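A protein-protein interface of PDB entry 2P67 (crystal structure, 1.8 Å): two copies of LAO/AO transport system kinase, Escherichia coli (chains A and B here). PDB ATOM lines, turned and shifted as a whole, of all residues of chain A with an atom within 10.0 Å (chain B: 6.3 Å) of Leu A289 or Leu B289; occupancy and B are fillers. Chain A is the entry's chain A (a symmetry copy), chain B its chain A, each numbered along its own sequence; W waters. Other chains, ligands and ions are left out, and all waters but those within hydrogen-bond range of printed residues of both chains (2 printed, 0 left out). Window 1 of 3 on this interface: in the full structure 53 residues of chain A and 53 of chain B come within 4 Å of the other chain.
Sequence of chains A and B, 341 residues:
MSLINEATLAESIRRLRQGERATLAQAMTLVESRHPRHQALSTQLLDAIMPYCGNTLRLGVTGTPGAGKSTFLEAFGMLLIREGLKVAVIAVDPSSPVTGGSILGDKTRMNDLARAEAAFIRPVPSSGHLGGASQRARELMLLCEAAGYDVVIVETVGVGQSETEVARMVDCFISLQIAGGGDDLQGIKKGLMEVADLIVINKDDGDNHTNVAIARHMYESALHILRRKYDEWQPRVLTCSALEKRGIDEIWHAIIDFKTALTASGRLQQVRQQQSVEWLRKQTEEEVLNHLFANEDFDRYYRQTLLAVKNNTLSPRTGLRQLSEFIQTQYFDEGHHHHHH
Among the printed residues, pairs that only touch across the chains: Tyr A302 with Arg B281 (3.2 Å), Arg A281 with Phe B293 (3.4 Å), Phe A293 with Arg B281 (3.4 Å), Glu A285 with Leu B289 (3.7 Å), Leu A289 with Glu B285 (3.7 Å), Ile A327 with Val B288 (3.8 Å), Gln A328 with His B291 (3.9 Å), Leu A292 with Val B288 (3.9 Å), Val A288 with Leu B292 (3.9 Å), Leu A289 with Leu B289 (3.9 Å), Phe A293 with Glu B285 (3.98 Å) and Glu A285 with Phe B293 (3.98 Å).
NE of Arg B281 lies within salt-bridge range of OE2 of Glu B285, 2.7 Å away.
The backbone carbonyl oxygen of Glu B287 is in hydrogen-bond range of a ring nitrogen (ND1) of His B291 (3.2 Å).
NE of Arg A281 is in salt-bridge range of OE2 of Glu A285 (2.7 Å).
The side-chain hydroxyl (OG) of Ser A324 sits at hydrogen-bond distance from the side-chain carboxylate (OE2) of Glu B287, 2.9 Å away.
Of the 12 printed residues of chain B, 8 touch a printed residue of chain A.
Hydrophobic or aromatic side chains of chain B that line the printed part of chain A: Val B288, Leu B289, His B291, Leu B292 and Phe B293.
Along chain A the printed residues that touch a printed residue of chain B span positions 281 to 328.
Among the printed residues, no Asp or Glu carboxylate lies within 4 Å of a Lys or Arg side-chain nitrogen of the other chain.
Water W1 bridges a ring nitrogen (ND1) of His B291 and the side-chain amide nitrogen of Gln A328.
Water W2 bridges the side-chain hydroxyl of Tyr A302 and the guanidinium group of Arg B281.
Arg A281 touches Phe B293, and with the chains exchanged Phe A293 touches Arg B281.
Glu A285 touches Phe B293, and with the chains exchanged Phe A293 touches Glu B285.
Val A288 touches Leu B292, and with the chains exchanged Leu A292 touches Val B288.
Leu A289 touches its own counterpart, Leu B289.
Positions printed for both chains: 281, 284, 285, 286, 287, 288, 289, 290, 291, 292, 293 and 294.
Lys A282 touches none of the printed residues of chain B.
Of the printed residues of chain B, Val A288 touches Leu B292 (3.9 Å).
Of chain B, only Glu B285 (3.7 Å) and Leu B289 (3.9 Å) come within 4 Å of Leu A289.
Ala A294 touches none of the printed residues of chain B.
Of the printed residues of chain B, Ser A324 touches Glu B287 (2.9 Å).
Printed residues of chain A within 4 Å of Arg B281: Phe A293 and Tyr A302.
Printed residues of chain A within 4 Å of Glu B287: Ser A324 (2.9 Å).
Of chain A, only Leu A292 and Ile A327 come within 4 Å of Val B288.
Of chain A, only Glu A285 (3.7 Å) and Leu A289 (3.9 Å) come within 4 Å of Leu B289.
No residue of chain A comes within 4 Å of Asn B290.
Printed residues of chain A within 4 Å of Phe B293: Arg A281 (3.4 Å) and Glu A285 (3.98 Å).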
ATOM      1  N   LEU A 280      37.950  -4.272 -21.804  1.00  0.00           N
ATOM      2  CA  LEU A 280      37.557  -5.609 -21.360  1.00  0.00           C
ATOM      3  C   LEU A 280      37.053  -5.609 -19.905  1.00  0.00           C
ATOM      4  O   LEU A 280      36.015  -6.190 -19.601  1.00  0.00           O
ATOM      5  CB  LEU A 280      38.729  -6.585 -21.497  1.00  0.00           C
ATOM      6  CG  LEU A 280      38.956  -7.203 -22.877  1.00  0.00           C
ATOM      7  CD1 LEU A 280      40.373  -7.825 -22.986  1.00  0.00           C
ATOM      8  CD2 LEU A 280      37.885  -8.239 -23.145  1.00  0.00           C
ATOM      9  N   ARG A 281      37.792  -4.947 -19.021  1.00  0.00           N
ATOM     10  CA  ARG A 281      37.459  -4.904 -17.610  1.00  0.00           C
ATOM     11  C   ARG A 281      36.134  -4.169 -17.406  1.00  0.00           C
ATOM     12  O   ARG A 281      35.226  -4.691 -16.753  1.00  0.00           O
ATOM     13  CB  ARG A 281      38.599  -4.231 -16.836  1.00  0.00           C
ATOM     14  CG  ARG A 281      38.395  -4.097 -15.323  1.00  0.00           C
ATOM     15  CD  ARG A 281      38.129  -5.437 -14.656  1.00  0.00           C
ATOM     16  NE  ARG A 281      38.059  -5.332 -13.199  1.00  0.00           N
ATOM     17  CZ  ARG A 281      39.030  -5.703 -12.370  1.00  0.00           C
ATOM     18  NH1 ARG A 281      40.171  -6.207 -12.847  1.00  0.00           N
ATOM     19  NH2 ARG A 281      38.858  -5.576 -11.060  1.00  0.00           N
ATOM     20  N   LYS A 282      36.022  -2.966 -17.973  1.00  0.00           N
ATOM     21  CA  LYS A 282      34.808  -2.170 -17.814  1.00  0.00           C
ATOM     22  C   LYS A 282      33.574  -2.879 -18.390  1.00  0.00           C
ATOM     23  O   LYS A 282      32.523  -2.915 -17.750  1.00  0.00           O
ATOM     24  CB  LYS A 282      34.975  -0.755 -18.387  1.00  0.00           C
ATOM     25  CG  LYS A 282      33.882   0.246 -17.957  1.00  0.00           C
ATOM     26  CD  LYS A 282      33.736   0.328 -16.431  1.00  0.00           C
ATOM     27  CE  LYS A 282      32.784   1.429 -15.998  1.00  0.00           C
ATOM     28  NZ  LYS A 282      32.894   1.705 -14.544  1.00  0.00           N
ATOM     29  N   GLN A 283      33.696  -3.477 -19.574  1.00  0.00           N
ATOM     30  CA  GLN A 283      32.533  -4.153 -20.150  1.00  0.00           C
ATOM     31  C   GLN A 283      32.120  -5.389 -19.356  1.00  0.00           C
ATOM     32  O   GLN A 283      30.934  -5.682 -19.240  1.00  0.00           O
ATOM     33  CB  GLN A 283      32.748  -4.493 -21.630  1.00  0.00           C
ATOM     34  CG  GLN A 283      32.925  -3.271 -22.527  1.00  0.00           C
ATOM     35  CD  GLN A 283      31.732  -2.321 -22.518  1.00  0.00           C
ATOM     36  OE1 GLN A 283      31.800  -1.234 -21.950  1.00  0.00           O
ATOM     37  NE2 GLN A 283      30.641  -2.724 -23.158  1.00  0.00           N
ATOM     38  N   THR A 284      33.097  -6.092 -18.796  1.00  0.00           N
ATOM     39  CA  THR A 284      32.833  -7.278 -17.977  1.00  0.00           C
ATOM     40  C   THR A 284      32.090  -6.875 -16.700  1.00  0.00           C
ATOM     41  O   THR A 284      31.044  -7.450 -16.362  1.00  0.00           O
ATOM     42  CB  THR A 284      34.137  -8.008 -17.624  1.00  0.00           C
ATOM     43  OG1 THR A 284      34.754  -8.464 -18.834  1.00  0.00           O
ATOM     44  CG2 THR A 284      33.876  -9.211 -16.698  1.00  0.00           C
ATOM     45  N   GLU A 285      32.627  -5.867 -16.016  1.00  0.00           N
ATOM     46  CA  GLU A 285      31.971  -5.311 -14.833  1.00  0.00           C
ATOM     47  C   GLU A 285      30.560  -4.815 -15.134  1.00  0.00           C
ATOM     48  O   GLU A 285      29.627  -5.110 -14.386  1.00  0.00           O
ATOM     49  CB  GLU A 285      32.793  -4.162 -14.257  1.00  0.00           C
ATOM     50  CG  GLU A 285      34.083  -4.584 -13.581  1.00  0.00           C
ATOM     51  CD  GLU A 285      34.903  -3.398 -13.132  1.00  0.00           C
ATOM     52  OE1 GLU A 285      34.441  -2.245 -13.314  1.00  0.00           O
ATOM     53  OE2 GLU A 285      36.006  -3.609 -12.591  1.00  0.00           O
ATOM     54  N   GLU A 286      30.410  -4.067 -16.226  1.00  0.00           N
ATOM     55  CA  GLU A 286      29.142  -3.404 -16.557  1.00  0.00           C
ATOM     56  C   GLU A 286      28.035  -4.377 -16.929  1.00  0.00           C
ATOM     57  O   GLU A 286      26.867  -4.115 -16.665  1.00  0.00           O
ATOM     58  CB  GLU A 286      29.320  -2.354 -17.655  1.00  0.00           C
ATOM     59  CG  GLU A 286      29.943  -1.054 -17.158  1.00  0.00           C
ATOM     60  CD  GLU A 286      29.940   0.063 -18.207  1.00  0.00           C
ATOM     61  OE1 GLU A 286      29.303  -0.101 -19.276  1.00  0.00           O
ATOM     62  OE2 GLU A 286      30.582   1.112 -17.959  1.00  0.00           O
ATOM     63  N   GLU A 287      28.406  -5.500 -17.540  1.00  0.00           N
ATOM     64  CA  GLU A 287      27.445  -6.555 -17.840  1.00  0.00           C
ATOM     65  C   GLU A 287      26.916  -7.195 -16.551  1.00  0.00           C
ATOM     66  O   GLU A 287      25.698  -7.331 -16.382  1.00  0.00           O
ATOM     67  CB  GLU A 287      28.064  -7.601 -18.772  1.00  0.00           C
ATOM     68  CG  GLU A 287      27.287  -8.904 -18.850  1.00  0.00           C
ATOM     69  CD  GLU A 287      27.247  -9.504 -20.245  1.00  0.00           C
ATOM     70  OE1 GLU A 287      27.551  -8.792 -21.235  1.00  0.00           O
ATOM     71  OE2 GLU A 287      26.888 -10.701 -20.348  1.00  0.00           O
ATOM     72  N   VAL A 288      27.833  -7.579 -15.660  1.00  0.00           N
ATOM     73  CA  VAL A 288      27.499  -8.125 -14.338  1.00  0.00           C
ATOM     74  C   VAL A 288      26.583  -7.167 -13.551  1.00  0.00           C
ATOM     75  O   VAL A 288      25.552  -7.581 -13.008  1.00  0.00           O
ATOM     76  CB  VAL A 288      28.773  -8.428 -13.510  1.00  0.00           C
ATOM     77  CG1 VAL A 288      28.420  -8.829 -12.069  1.00  0.00           C
ATOM     78  CG2 VAL A 288      29.577  -9.520 -14.164  1.00  0.00           C
ATOM     79  N   LEU A 289      26.964  -5.894 -13.508  1.00  0.00           N
ATOM     80  CA  LEU A 289      26.184  -4.877 -12.796  1.00  0.00           C
ATOM     81  C   LEU A 289      24.825  -4.579 -13.445  1.00  0.00           C
ATOM     82  O   LEU A 289      23.818  -4.461 -12.742  1.00  0.00           O
ATOM     83  CB  LEU A 289      27.002  -3.597 -12.624  1.00  0.00           C
ATOM     84  CG  LEU A 289      28.263  -3.747 -11.774  1.00  0.00           C
ATOM     85  CD1 LEU A 289      28.926  -2.397 -11.618  1.00  0.00           C
ATOM     86  CD2 LEU A 289      27.928  -4.340 -10.431  1.00  0.00           C
ATOM     87  N   ASN A 290      24.800  -4.471 -14.776  1.00  0.00           N
ATOM     88  CA  ASN A 290      23.547  -4.251 -15.510  1.00  0.00           C
ATOM     89  C   ASN A 290      22.530  -5.363 -15.326  1.00  0.00           C
ATOM     90  O   ASN A 290      21.327  -5.099 -15.249  1.00  0.00           O
ATOM     91  CB  ASN A 290      23.800  -4.025 -17.002  1.00  0.00           C
ATOM     92  CG  ASN A 290      24.223  -2.602 -17.313  1.00  0.00           C
ATOM     93  OD1 ASN A 290      23.905  -1.667 -16.571  1.00  0.00           O
ATOM     94  ND2 ASN A 290      24.946  -2.427 -18.415  1.00  0.00           N
ATOM     95  N   HIS A 291      23.005  -6.603 -15.259  1.00  0.00           N
ATOM     96  CA  HIS A 291      22.113  -7.731 -15.027  1.00  0.00           C
ATOM     97  C   HIS A 291      21.466  -7.659 -13.649  1.00  0.00           C
ATOM     98  O   HIS A 291      20.267  -7.921 -13.503  1.00  0.00           O
ATOM     99  CB  HIS A 291      22.842  -9.063 -15.222  1.00  0.00           C
ATOM    100  CG  HIS A 291      23.003  -9.457 -16.660  1.00  0.00           C
ATOM    101  ND1 HIS A 291      24.163 -10.020 -17.153  1.00  0.00           N
ATOM    102  CD2 HIS A 291      22.155  -9.364 -17.714  1.00  0.00           C
ATOM    103  CE1 HIS A 291      24.019 -10.263 -18.445  1.00  0.00           C
ATOM    104  NE2 HIS A 291      22.813  -9.870 -18.811  1.00  0.00           N
ATOM    105  N   LEU A 292      22.264  -7.294 -12.648  1.00  0.00           N
ATOM    106  CA  LEU A 292      21.780  -7.110 -11.276  1.00  0.00           C
ATOM    107  C   LEU A 292      20.767  -5.965 -11.168  1.00  0.00           C
ATOM    108  O   LEU A 292      19.651  -6.166 -10.693  1.00  0.00           O
ATOM    109  CB  LEU A 292      22.960  -6.868 -10.330  1.00  0.00           C
ATOM    110  CG  LEU A 292      22.654  -6.706  -8.846  1.00  0.00           C
ATOM    111  CD1 LEU A 292      22.111  -8.004  -8.265  1.00  0.00           C
ATOM    112  CD2 LEU A 292      23.915  -6.263  -8.112  1.00  0.00           C
ATOM    113  N   PHE A 293      21.156  -4.777 -11.623  1.00  0.00           N
ATOM    114  CA  PHE A 293      20.308  -3.590 -11.502  1.00  0.00           C
ATOM    115  C   PHE A 293      19.128  -3.584 -12.481  1.00  0.00           C
ATOM    116  O   PHE A 293      18.178  -2.808 -12.320  1.00  0.00           O
ATOM    117  CB  PHE A 293      21.153  -2.311 -11.586  1.00  0.00           C
ATOM    118  CG  PHE A 293      21.995  -2.067 -10.351  1.00  0.00           C
ATOM    119  CD1 PHE A 293      23.229  -2.697 -10.191  1.00  0.00           C
ATOM    120  CD2 PHE A 293      21.538  -1.229  -9.337  1.00  0.00           C
ATOM    121  CE1 PHE A 293      23.997  -2.494  -9.040  1.00  0.00           C
ATOM    122  CE2 PHE A 293      22.300  -1.011  -8.183  1.00  0.00           C
ATOM    123  CZ  PHE A 293      23.527  -1.639  -8.034  1.00  0.00           C
ATOM    124  N   ALA A 294      19.179  -4.473 -13.474  1.00  0.00           N
ATOM    125  CA  ALA A 294      18.050  -4.687 -14.382  1.00  0.00           C
ATOM    126  C   ALA A 294      16.995  -5.583 -13.737  1.00  0.00           C
ATOM    127  O   ALA A 294      15.791  -5.371 -13.934  1.00  0.00           O
ATOM    128  CB  ALA A 294      18.518  -5.283 -15.710  1.00  0.00           C
ATOM    129  N   ASN A 295      17.450  -6.575 -12.973  1.00  0.00           N
ATOM    130  CA  ASN A 295      16.560  -7.472 -12.248  1.00  0.00           C
ATOM    131  C   ASN A 295      15.433  -6.699 -11.541  1.00  0.00           C
ATOM    132  O   ASN A 295      15.690  -5.758 -10.780  1.00  0.00           O
ATOM    133  CB  ASN A 295      17.352  -8.314 -11.253  1.00  0.00           C
ATOM    134  CG  ASN A 295      16.541  -9.454 -10.684  1.00  0.00           C
ATOM    135  OD1 ASN A 295      16.334 -10.469 -11.347  1.00  0.00           O
ATOM    136  ND2 ASN A 295      16.076  -9.298  -9.453  1.00  0.00           N
ATOM    137  N   PHE A 298      15.473  -7.017  -7.647  1.00  0.00           N
ATOM    138  CA  PHE A 298      16.580  -6.302  -7.026  1.00  0.00           C
ATOM    139  C   PHE A 298      16.411  -4.790  -7.137  1.00  0.00           C
ATOM    140  O   PHE A 298      16.720  -4.069  -6.195  1.00  0.00           O
ATOM    141  CB  PHE A 298      17.947  -6.712  -7.585  1.00  0.00           C
ATOM    142  CG  PHE A 298      19.076  -5.966  -6.947  1.00  0.00           C
ATOM    143  CD1 PHE A 298      19.540  -6.334  -5.684  1.00  0.00           C
ATOM    144  CD2 PHE A 298      19.629  -4.856  -7.567  1.00  0.00           C
ATOM    145  CE1 PHE A 298      20.575  -5.612  -5.061  1.00  0.00           C
ATOM    146  CE2 PHE A 298      20.657  -4.130  -6.950  1.00  0.00           C
ATOM    147  CZ  PHE A 298      21.125  -4.513  -5.701  1.00  0.00           C
ATOM    148  N   ASP A 299      15.958  -4.322  -8.297  1.00  0.00           N
ATOM    149  CA  ASP A 299      15.717  -2.899  -8.524  1.00  0.00           C
ATOM    150  C   ASP A 299      14.723  -2.360  -7.495  1.00  0.00           C
ATOM    151  O   ASP A 299      14.912  -1.267  -6.950  1.00  0.00           O
ATOM    152  CB  ASP A 299      15.198  -2.657  -9.946  1.00  0.00           C
ATOM    153  CG  ASP A 299      14.726  -1.230 -10.163  1.00  0.00           C
ATOM    154  OD1 ASP A 299      15.564  -0.310 -10.127  1.00  0.00           O
ATOM    155  OD2 ASP A 299      13.508  -1.027 -10.344  1.00  0.00           O
ATOM    156  N   TYR A 302      16.385  -2.459  -3.996  1.00  0.00           N
ATOM    157  CA  TYR A 302      17.384  -1.386  -3.999  1.00  0.00           C
ATOM    158  C   TYR A 302      16.740  -0.012  -3.783  1.00  0.00           C
ATOM    159  O   TYR A 302      17.217   0.786  -2.967  1.00  0.00           O
ATOM    160  CB  TYR A 302      18.213  -1.420  -5.300  1.00  0.00           C
ATOM    161  CG  TYR A 302      19.276  -0.356  -5.339  1.00  0.00           C
ATOM    162  CD1 TYR A 302      20.461  -0.505  -4.620  1.00  0.00           C
ATOM    163  CD2 TYR A 302      19.104   0.798  -6.100  1.00  0.00           C
ATOM    164  CE1 TYR A 302      21.453   0.487  -4.637  1.00  0.00           C
ATOM    165  CE2 TYR A 302      20.088   1.790  -6.129  1.00  0.00           C
ATOM    166  CZ  TYR A 302      21.251   1.628  -5.379  1.00  0.00           C
ATOM    167  OH  TYR A 302      22.215   2.604  -5.418  1.00  0.00           O
ATOM    168  N   SER A 324      23.614  -6.483   0.442  1.00  0.00           N
ATOM    169  CA  SER A 324      24.567  -7.590   0.292  1.00  0.00           C
ATOM    170  C   SER A 324      23.907  -8.937   0.557  1.00  0.00           C
ATOM    171  O   SER A 324      24.087  -9.890  -0.200  1.00  0.00           O
ATOM    172  CB  SER A 324      25.748  -7.420   1.245  1.00  0.00           C
ATOM    173  OG  SER A 324      26.547  -6.315   0.877  1.00  0.00           O
ATOM    174  N   ILE A 327      21.596  -9.879  -2.258  1.00  0.00           N
ATOM    175  CA  ILE A 327      22.398 -10.369  -3.387  1.00  0.00           C
ATOM    176  C   ILE A 327      22.914 -11.805  -3.179  1.00  0.00           C
ATOM    177  O   ILE A 327      22.787 -12.636  -4.080  1.00  0.00           O
ATOM    178  CB  ILE A 327      23.544  -9.389  -3.747  1.00  0.00           C
ATOM    179  CG1 ILE A 327      22.961  -8.104  -4.337  1.00  0.00           C
ATOM    180  CG2 ILE A 327      24.543 -10.029  -4.727  1.00  0.00           C
ATOM    181  CD1 ILE A 327      23.809  -6.893  -4.111  1.00  0.00           C
ATOM    182  N   GLN A 328      23.462 -12.086  -1.994  1.00  0.00           N
ATOM    183  CA  GLN A 328      23.961 -13.426  -1.641  1.00  0.00           C
ATOM    184  C   GLN A 328      22.858 -14.472  -1.709  1.00  0.00           C
ATOM    185  O   GLN A 328      23.076 -15.576  -2.200  1.00  0.00           O
ATOM    186  CB  GLN A 328      24.574 -13.446  -0.235  1.00  0.00           C
ATOM    187  CG  GLN A 328      25.737 -12.486  -0.014  1.00  0.00           C
ATOM    188  CD  GLN A 328      26.820 -12.626  -1.061  1.00  0.00           C
ATOM    189  OE1 GLN A 328      27.337 -13.726  -1.295  1.00  0.00           O
ATOM    190  NE2 GLN A 328      27.171 -11.509  -1.704  1.00  0.00           N
ATOM    191  N   ARG B 281      25.498   3.198  -3.787  1.00  0.00           N
ATOM    192  CA  ARG B 281      25.575   2.581  -5.098  1.00  0.00           C
ATOM    193  C   ARG B 281      26.979   2.023  -5.332  1.00  0.00           C
ATOM    194  O   ARG B 281      27.132   0.851  -5.690  1.00  0.00           O
ATOM    195  CB  ARG B 281      25.193   3.610  -6.169  1.00  0.00           C
ATOM    196  CG  ARG B 281      25.237   3.115  -7.620  1.00  0.00           C
ATOM    197  CD  ARG B 281      24.361   1.893  -7.838  1.00  0.00           C
ATOM    198  NE  ARG B 281      24.299   1.493  -9.244  1.00  0.00           N
ATOM    199  CZ  ARG B 281      23.268   1.728 -10.049  1.00  0.00           C
ATOM    200  NH1 ARG B 281      22.191   2.376  -9.597  1.00  0.00           N
ATOM    201  NH2 ARG B 281      23.311   1.310 -11.308  1.00  0.00           N
ATOM    202  N   THR B 284      27.817  -0.989  -3.079  1.00  0.00           N
ATOM    203  CA  THR B 284      27.031  -2.157  -3.486  1.00  0.00           C
ATOM    204  C   THR B 284      27.664  -2.806  -4.720  1.00  0.00           C
ATOM    205  O   THR B 284      27.913  -4.022  -4.745  1.00  0.00           O
ATOM    206  CB  THR B 284      25.574  -1.770  -3.780  1.00  0.00           C
ATOM    207  OG1 THR B 284      24.979  -1.264  -2.579  1.00  0.00           O
ATOM    208  CG2 THR B 284      24.761  -2.977  -4.284  1.00  0.00           C
ATOM    209  N   GLU B 285      27.945  -1.980  -5.725  1.00  0.00           N
ATOM    210  CA  GLU B 285      28.642  -2.444  -6.925  1.00  0.00           C
ATOM    211  C   GLU B 285      29.995  -3.071  -6.601  1.00  0.00           C
ATOM    212  O   GLU B 285      30.317  -4.145  -7.110  1.00  0.00           O
ATOM    213  CB  GLU B 285      28.846  -1.291  -7.903  1.00  0.00           C
ATOM    214  CG  GLU B 285      27.581  -0.813  -8.589  1.00  0.00           C
ATOM    215  CD  GLU B 285      27.829   0.397  -9.457  1.00  0.00           C
ATOM    216  OE1 GLU B 285      29.000   0.837  -9.554  1.00  0.00           O
ATOM    217  OE2 GLU B 285      26.861   0.911 -10.051  1.00  0.00           O
ATOM    218  N   GLU B 286      30.777  -2.399  -5.757  1.00  0.00           N
ATOM    219  CA  GLU B 286      32.158  -2.810  -5.471  1.00  0.00           C
ATOM    220  C   GLU B 286      32.249  -4.116  -4.699  1.00  0.00           C
ATOM    221  O   GLU B 286      33.196  -4.873  -4.877  1.00  0.00           O
ATOM    222  CB  GLU B 286      32.938  -1.709  -4.749  1.00  0.00           C
ATOM    223  CG  GLU B 286      33.397  -0.584  -5.670  1.00  0.00           C
ATOM    224  CD  GLU B 286      34.342   0.412  -4.991  1.00  0.00           C
ATOM    225  OE1 GLU B 286      34.789   0.152  -3.848  1.00  0.00           O
ATOM    226  OE2 GLU B 286      34.636   1.465  -5.606  1.00  0.00           O
ATOM    227  N   GLU B 287      31.261  -4.377  -3.847  1.00  0.00           N
ATOM    228  CA  GLU B 287      31.185  -5.650  -3.139  1.00  0.00           C
ATOM    229  C   GLU B 287      30.914  -6.802  -4.115  1.00  0.00           C
ATOM    230  O   GLU B 287      31.619  -7.819  -4.083  1.00  0.00           O
ATOM    231  CB  GLU B 287      30.125  -5.592  -2.035  1.00  0.00           C
ATOM    232  CG  GLU B 287      29.716  -6.950  -1.491  1.00  0.00           C
ATOM    233  CD  GLU B 287      29.485  -6.959   0.011  1.00  0.00           C
ATOM    234  OE1 GLU B 287      29.921  -6.010   0.710  1.00  0.00           O
ATOM    235  OE2 GLU B 287      28.873  -7.940   0.495  1.00  0.00           O
ATOM    236  N   VAL B 288      29.902  -6.631  -4.968  1.00  0.00           N
ATOM    237  CA  VAL B 288      29.565  -7.593  -6.027  1.00  0.00           C
ATOM    238  C   VAL B 288      30.779  -7.880  -6.931  1.00  0.00           C
ATOM    239  O   VAL B 288      31.108  -9.041  -7.199  1.00  0.00           O
ATOM    240  CB  VAL B 288      28.378  -7.094  -6.889  1.00  0.00           C
ATOM    241  CG1 VAL B 288      28.143  -8.011  -8.100  1.00  0.00           C
ATOM    242  CG2 VAL B 288      27.124  -7.010  -6.059  1.00  0.00           C
ATOM    243  N   LEU B 289      31.440  -6.817  -7.383  1.00  0.00           N
ATOM    244  CA  LEU B 289      32.615  -6.948  -8.249  1.00  0.00           C
ATOM    245  C   LEU B 289      33.832  -7.562  -7.545  1.00  0.00           C
ATOM    246  O   LEU B 289      34.511  -8.418  -8.119  1.00  0.00           O
ATOM    247  CB  LEU B 289      32.967  -5.602  -8.881  1.00  0.00           C
ATOM    248  CG  LEU B 289      31.897  -5.023  -9.806  1.00  0.00           C
ATOM    249  CD1 LEU B 289      32.408  -3.741 -10.423  1.00  0.00           C
ATOM    250  CD2 LEU B 289      31.524  -6.019 -10.871  1.00  0.00           C
ATOM    251  N   ASN B 290      34.097  -7.134  -6.308  1.00  0.00           N
ATOM    252  CA  ASN B 290      35.198  -7.696  -5.515  1.00  0.00           C
ATOM    253  C   ASN B 290      35.056  -9.183  -5.244  1.00  0.00           C
ATOM    254  O   ASN B 290      36.052  -9.912  -5.239  1.00  0.00           O
ATOM    255  CB  ASN B 290      35.379  -6.945  -4.193  1.00  0.00           C
ATOM    256  CG  ASN B 290      36.165  -5.659  -4.356  1.00  0.00           C
ATOM    257  OD1 ASN B 290      36.964  -5.514  -5.287  1.00  0.00           O
ATOM    258  ND2 ASN B 290      35.942  -4.711  -3.451  1.00  0.00           N
ATOM    259  N   HIS B 291      33.827  -9.635  -5.014  1.00  0.00           N
ATOM    260  CA  HIS B 291      33.583 -11.055  -4.801  1.00  0.00           C
ATOM    261  C   HIS B 291      33.899 -11.871  -6.049  1.00  0.00           C
ATOM    262  O   HIS B 291      34.501 -12.947  -5.961  1.00  0.00           O
ATOM    263  CB  HIS B 291      32.149 -11.306  -4.330  1.00  0.00           C
ATOM    264  CG  HIS B 291      31.936 -11.027  -2.872  1.00  0.00           C
ATOM    265  ND1 HIS B 291      30.806 -10.398  -2.390  1.00  0.00           N
ATOM    266  CD2 HIS B 291      32.711 -11.283  -1.789  1.00  0.00           C
ATOM    267  CE1 HIS B 291      30.890 -10.288  -1.075  1.00  0.00           C
ATOM    268  NE2 HIS B 291      32.039 -10.811  -0.686  1.00  0.00           N
ATOM    269  N   LEU B 292      33.497 -11.349  -7.206  1.00  0.00           N
ATOM    270  CA  LEU B 292      33.784 -11.975  -8.500  1.00  0.00           C
ATOM    271  C   LEU B 292      35.285 -12.022  -8.800  1.00  0.00           C
ATOM    272  O   LEU B 292      35.835 -13.092  -9.053  1.00  0.00           O
ATOM    273  CB  LEU B 292      33.040 -11.236  -9.617  1.00  0.00           C
ATOM    274  CG  LEU B 292      33.176 -11.779 -11.035  1.00  0.00           C
ATOM    275  CD1 LEU B 292      32.529 -13.151 -11.149  1.00  0.00           C
ATOM    276  CD2 LEU B 292      32.551 -10.796 -12.018  1.00  0.00           C
ATOM    277  N   PHE B 293      35.941 -10.865  -8.756  1.00  0.00           N
ATOM    278  CA  PHE B 293      37.360 -10.770  -9.100  1.00  0.00           C
ATOM    279  C   PHE B 293      38.288 -11.344  -8.022  1.00  0.00           C
ATOM    280  O   PHE B 293      39.474 -11.592  -8.276  1.00  0.00           O
ATOM    281  CB  PHE B 293      37.726  -9.332  -9.491  1.00  0.00           C
ATOM    282  CG  PHE B 293      37.177  -8.920 -10.841  1.00  0.00           C
ATOM    283  CD1 PHE B 293      35.865  -8.466 -10.971  1.00  0.00           C
ATOM    284  CD2 PHE B 293      37.966  -9.015 -11.986  1.00  0.00           C
ATOM    285  CE1 PHE B 293      35.347  -8.109 -12.219  1.00  0.00           C
ATOM    286  CE2 PHE B 293      37.461  -8.653 -13.241  1.00  0.00           C
ATOM    287  CZ  PHE B 293      36.157  -8.200 -13.359  1.00  0.00           C
ATOM    288  N   ALA B 294      37.734 -11.582  -6.832  1.00  0.00           N
ATOM    289  CA  ALA B 294      38.459 -12.276  -5.765  1.00  0.00           C
ATOM    290  C   ALA B 294      38.442 -13.787  -5.989  1.00  0.00           C
ATOM    291  O   ALA B 294      39.435 -14.471  -5.709  1.00  0.00           O
ATOM    292  CB  ALA B 294      37.878 -11.932  -4.393  1.00  0.00           C
HETATM  293  O   HOH W   1      28.628 -10.665  -4.095  1.00  0.00           O
HETATM  294  O   HOH W   2      21.633   4.531  -7.545  1.00  0.00           O
